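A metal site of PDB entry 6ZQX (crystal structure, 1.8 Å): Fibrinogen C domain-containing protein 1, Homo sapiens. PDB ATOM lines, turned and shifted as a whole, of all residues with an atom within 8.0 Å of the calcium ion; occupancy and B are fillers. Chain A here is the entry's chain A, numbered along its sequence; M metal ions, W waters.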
ATOM      1  N   THR A 153      29.467 -19.365  -5.567  1.00  0.00           N
ATOM      2  CA  THR A 153      28.885 -18.945  -6.861  1.00  0.00           C
ATOM      3  C   THR A 153      29.728 -17.800  -7.440  1.00  0.00           C
ATOM      4  O   THR A 153      30.033 -16.844  -6.711  1.00  0.00           O
ATOM      5  CB  THR A 153      27.397 -18.577  -6.643  1.00  0.00           C
ATOM      6  OG1 THR A 153      26.636 -19.779  -6.573  1.00  0.00           O
ATOM      7  CG2 THR A 153      26.829 -17.716  -7.745  1.00  0.00           C
ATOM      8  N   ARG A 157      29.282 -19.487 -12.971  1.00  0.00           N
ATOM      9  CA  ARG A 157      28.912 -20.796 -12.360  1.00  0.00           C
ATOM     10  C   ARG A 157      27.972 -20.589 -11.180  1.00  0.00           C
ATOM     11  O   ARG A 157      28.430 -20.309 -10.026  1.00  0.00           O
ATOM     12  CB  ARG A 157      30.150 -21.581 -11.915  1.00  0.00           C
ATOM     13  CG  ARG A 157      29.873 -23.063 -11.670  1.00  0.00           C
ATOM     14  CD  ARG A 157      31.132 -23.756 -11.180  1.00  0.00           C
ATOM     15  NE  ARG A 157      31.020 -25.207 -11.108  1.00  0.00           N
ATOM     16  CZ  ARG A 157      30.545 -25.892 -10.084  1.00  0.00           C
ATOM     17  NH1 ARG A 157      30.075 -25.282  -9.008  1.00  0.00           N
ATOM     18  NH2 ARG A 157      30.484 -27.214 -10.144  1.00  0.00           N
ATOM     19  N   ASP A 158      26.680 -20.794 -11.436  1.00  0.00           N
ATOM     20  CA  ASP A 158      25.581 -20.427 -10.520  1.00  0.00           C
ATOM     21  C   ASP A 158      25.173 -21.654  -9.683  1.00  0.00           C
ATOM     22  O   ASP A 158      24.629 -22.579 -10.289  1.00  0.00           O
ATOM     23  CB  ASP A 158      24.411 -19.892 -11.341  1.00  0.00           C
ATOM     24  CG  ASP A 158      23.220 -19.433 -10.531  1.00  0.00           C
ATOM     25  OD1 ASP A 158      23.116 -19.814  -9.342  1.00  0.00           O
ATOM     26  OD2 ASP A 158      22.406 -18.664 -11.098  1.00  0.00           O
ATOM     27  N   SER A 159      25.350 -21.604  -8.358  1.00  0.00           N
ATOM     28  CA  SER A 159      24.919 -22.656  -7.398  1.00  0.00           C
ATOM     29  C   SER A 159      24.110 -22.032  -6.250  1.00  0.00           C
ATOM     30  O   SER A 159      24.018 -22.673  -5.192  1.00  0.00           O
ATOM     31  CB  SER A 159      26.092 -23.427  -6.875  1.00  0.00           C
ATOM     32  OG  SER A 159      26.835 -23.991  -7.940  1.00  0.00           O
ATOM     33  N   ASP A 160      23.556 -20.837  -6.434  1.00  0.00           N
ATOM     34  CA  ASP A 160      22.899 -20.080  -5.347  1.00  0.00           C
ATOM     35  C   ASP A 160      21.411 -20.479  -5.300  1.00  0.00           C
ATOM     36  O   ASP A 160      21.009 -21.383  -6.067  1.00  0.00           O
ATOM     37  CB  ASP A 160      23.127 -18.569  -5.520  1.00  0.00           C
ATOM     38  CG  ASP A 160      22.538 -18.008  -6.796  1.00  0.00           C
ATOM     39  OD1 ASP A 160      21.386 -18.404  -7.135  1.00  0.00           O
ATOM     40  OD2 ASP A 160      23.249 -17.203  -7.469  1.00  0.00           O
ATOM     41  N   HIS A 161      20.642 -19.847  -4.397  1.00  0.00           N
ATOM     42  CA  HIS A 161      19.191 -20.103  -4.207  1.00  0.00           C
ATOM     43  C   HIS A 161      18.371 -18.969  -4.827  1.00  0.00           C
ATOM     44  O   HIS A 161      17.236 -18.718  -4.369  1.00  0.00           O
ATOM     45  CB  HIS A 161      18.879 -20.332  -2.731  1.00  0.00           C
ATOM     46  CG  HIS A 161      19.346 -21.653  -2.232  1.00  0.00           C
ATOM     47  ND1 HIS A 161      19.183 -22.046  -0.926  1.00  0.00           N
ATOM     48  CD2 HIS A 161      20.003 -22.661  -2.856  1.00  0.00           C
ATOM     49  CE1 HIS A 161      19.693 -23.250  -0.752  1.00  0.00           C
ATOM     50  NE2 HIS A 161      20.213 -23.651  -1.930  1.00  0.00           N
ATOM     51  N   SER A 162      18.887 -18.329  -5.860  1.00  0.00           N
ATOM     52  CA  SER A 162      18.232 -17.182  -6.532  1.00  0.00           C
ATOM     53  C   SER A 162      17.866 -17.587  -7.955  1.00  0.00           C
ATOM     54  O   SER A 162      18.616 -18.381  -8.528  1.00  0.00           O
ATOM     55  CB  SER A 162      19.111 -15.951  -6.509  1.00  0.00           C
ATOM     56  OG  SER A 162      18.489 -14.904  -7.229  1.00  0.00           O
ATOM     57  N   GLU A 163      16.773 -17.030  -8.487  1.00  0.00           N
ATOM     58  CA  GLU A 163      16.300 -17.239  -9.888  1.00  0.00           C
ATOM     59  C   GLU A 163      17.332 -16.661 -10.856  1.00  0.00           C
ATOM     60  O   GLU A 163      17.449 -17.172 -11.986  1.00  0.00           O
ATOM     61  CB  GLU A 163      14.924 -16.612 -10.083  1.00  0.00           C
ATOM     62  CG  GLU A 163      13.811 -17.381  -9.386  1.00  0.00           C
ATOM     63  CD  GLU A 163      12.518 -16.617  -9.087  1.00  0.00           C
ATOM     64  OE1 GLU A 163      12.568 -15.367  -8.994  1.00  0.00           O
ATOM     65  OE2 GLU A 163      11.465 -17.282  -8.940  1.00  0.00           O
ATOM     66  N   ASN A 164      18.105 -15.647 -10.422  1.00  0.00           N
ATOM     67  CA  ASN A 164      19.237 -15.120 -11.223  1.00  0.00           C
ATOM     68  C   ASN A 164      20.561 -15.502 -10.535  1.00  0.00           C
ATOM     69  O   ASN A 164      20.579 -16.319  -9.585  1.00  0.00           O
ATOM     70  CB  ASN A 164      19.097 -13.617 -11.530  1.00  0.00           C
ATOM     71  CG  ASN A 164      18.698 -12.793 -10.335  1.00  0.00           C
ATOM     72  OD1 ASN A 164      17.501 -12.661 -10.044  1.00  0.00           O
ATOM     73  ND2 ASN A 164      19.676 -12.215  -9.659  1.00  0.00           N
ATOM     74  N   ASN A 165      21.656 -14.993 -11.096  1.00  0.00           N
ATOM     75  CA  ASN A 165      23.029 -15.282 -10.617  1.00  0.00           C
ATOM     76  C   ASN A 165      23.430 -14.156  -9.636  1.00  0.00           C
ATOM     77  O   ASN A 165      23.678 -13.027 -10.096  1.00  0.00           O
ATOM     78  CB  ASN A 165      23.976 -15.447 -11.799  1.00  0.00           C
ATOM     79  CG  ASN A 165      25.382 -15.789 -11.364  1.00  0.00           C
ATOM     80  OD1 ASN A 165      25.877 -15.238 -10.395  1.00  0.00           O
ATOM     81  ND2 ASN A 165      26.027 -16.690 -12.094  1.00  0.00           N
ATOM     82  N   CYS A 166      23.505 -14.485  -8.351  1.00  0.00           N
ATOM     83  CA  CYS A 166      23.815 -13.546  -7.245  1.00  0.00           C
ATOM     84  C   CYS A 166      25.173 -12.877  -7.511  1.00  0.00           C
ATOM     85  O   CYS A 166      25.305 -11.656  -7.204  1.00  0.00           O
ATOM     86  CB  CYS A 166      23.817 -14.254  -5.905  1.00  0.00           C
ATOM     87  SG  CYS A 166      22.186 -14.755  -5.286  1.00  0.00           S
ATOM     88  N   ALA A 167      26.157 -13.616  -8.028  1.00  0.00           N
ATOM     89  CA  ALA A 167      27.524 -13.111  -8.297  1.00  0.00           C
ATOM     90  C   ALA A 167      27.475 -12.019  -9.381  1.00  0.00           C
ATOM     91  O   ALA A 167      28.127 -10.968  -9.208  1.00  0.00           O
ATOM     92  CB  ALA A 167      28.453 -14.238  -8.686  1.00  0.00           C
ATOM     93  N   TYR A 176      26.728 -17.443  -1.900  1.00  0.00           N
ATOM     94  CA  TYR A 176      25.455 -16.698  -2.010  1.00  0.00           C
ATOM     95  C   TYR A 176      24.267 -17.629  -1.721  1.00  0.00           C
ATOM     96  O   TYR A 176      24.266 -18.799  -2.156  1.00  0.00           O
ATOM     97  CB  TYR A 176      25.320 -16.067  -3.398  1.00  0.00           C
ATOM     98  CG  TYR A 176      26.271 -14.940  -3.726  1.00  0.00           C
ATOM     99  CD1 TYR A 176      26.182 -13.728  -3.079  1.00  0.00           C
ATOM    100  CD2 TYR A 176      27.219 -15.068  -4.739  1.00  0.00           C
ATOM    101  CE1 TYR A 176      27.007 -12.670  -3.405  1.00  0.00           C
ATOM    102  CE2 TYR A 176      28.055 -14.005  -5.072  1.00  0.00           C
ATOM    103  CZ  TYR A 176      27.948 -12.794  -4.412  1.00  0.00           C
ATOM    104  OH  TYR A 176      28.773 -11.746  -4.716  1.00  0.00           O
ATOM    105  N   ARG A 177      23.285 -17.114  -0.991  1.00  0.00           N
ATOM    106  CA  ARG A 177      21.947 -17.751  -0.831  1.00  0.00           C
ATOM    107  C   ARG A 177      20.993 -17.006  -1.770  1.00  0.00           C
ATOM    108  O   ARG A 177      20.914 -17.367  -2.960  1.00  0.00           O
ATOM    109  CB  ARG A 177      21.533 -17.765   0.645  1.00  0.00           C
ATOM    110  CG  ARG A 177      20.171 -18.397   0.902  1.00  0.00           C
ATOM    111  CD  ARG A 177      19.812 -18.384   2.373  1.00  0.00           C
ATOM    112  NE  ARG A 177      20.815 -19.102   3.157  1.00  0.00           N
ATOM    113  CZ  ARG A 177      20.820 -20.418   3.414  1.00  0.00           C
ATOM    114  NH1 ARG A 177      19.857 -21.204   2.958  1.00  0.00           N
ATOM    115  NH2 ARG A 177      21.795 -20.929   4.140  1.00  0.00           N
ATOM    116  N   ASN A 178      20.328 -15.951  -1.278  1.00  0.00           N
ATOM    117  CA  ASN A 178      19.324 -15.211  -2.092  1.00  0.00           C
ATOM    118  C   ASN A 178      19.172 -13.786  -1.579  1.00  0.00           C
ATOM    119  O   ASN A 178      18.084 -13.425  -1.152  1.00  0.00           O
ATOM    120  CB  ASN A 178      17.977 -15.937  -2.063  1.00  0.00           C
ATOM    121  CG  ASN A 178      16.975 -15.360  -3.030  1.00  0.00           C
ATOM    122  OD1 ASN A 178      17.329 -14.964  -4.137  1.00  0.00           O
ATOM    123  ND2 ASN A 178      15.708 -15.336  -2.623  1.00  0.00           N
ATOM    124  N   CYS A 179      20.256 -12.985  -1.569  1.00  0.00           N
ATOM    125  CA  CYS A 179      21.571 -13.345  -2.071  1.00  0.00           C
ATOM    126  C   CYS A 179      22.631 -13.290  -0.963  1.00  0.00           C
ATOM    127  O   CYS A 179      23.420 -14.260  -0.854  1.00  0.00           O
ATOM    128  CB  CYS A 179      21.999 -12.444  -3.227  1.00  0.00           C
ATOM    129  SG  CYS A 179      21.244 -12.914  -4.803  1.00  0.00           S
HETATM  130 CA    CA M   1      20.812 -18.736  -9.311  1.00  0.00          CA
HETATM  131  O   HOH W   1      19.596 -19.638 -11.306  1.00  0.00           O
HETATM  132  O   HOH W   2      20.368 -20.963  -8.780  1.00  0.00           O
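Of the 16 residues printed, 4 come within 4 Å of the calcium ion. Along chain A the residues within 4 Å of the calcium ion span positions 158 to 164.
The side-chain hydroxyl (OG) of Ser 162 lies close to the side-chain amide oxygen (OD1) of Asn 178, at 3.3 Å. OD2 of Asp 160 sits at hydrogen-bond distance from N of Cys 166 (2.9 Å). The backbone NH (N) of Asp 160 lies within hydrogen-bond range of the side-chain hydroxyl (OG1) of Thr 153 (3.3 Å). The side-chain sulfur (SG) of Cys 166 forms a disulfide with the side-chain sulfur (SG) of Cys 179 (2.1 Å). OG of Ser 162 lies close to N of Asn 164, 3.3 Å away.
The calcium ion is bound by OD1 of Asp 160 (2.3 Å), water W2 (2.3 Å), O of Ser 162 (2.4 Å), OD2 of Asp 158 (2.4 Å), O of Asn 164 (2.4 Å), water W1 (2.5 Å) and OD1 of Asp 158 (2.5 Å). The calcium ion has seven donor atoms within binding distance.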
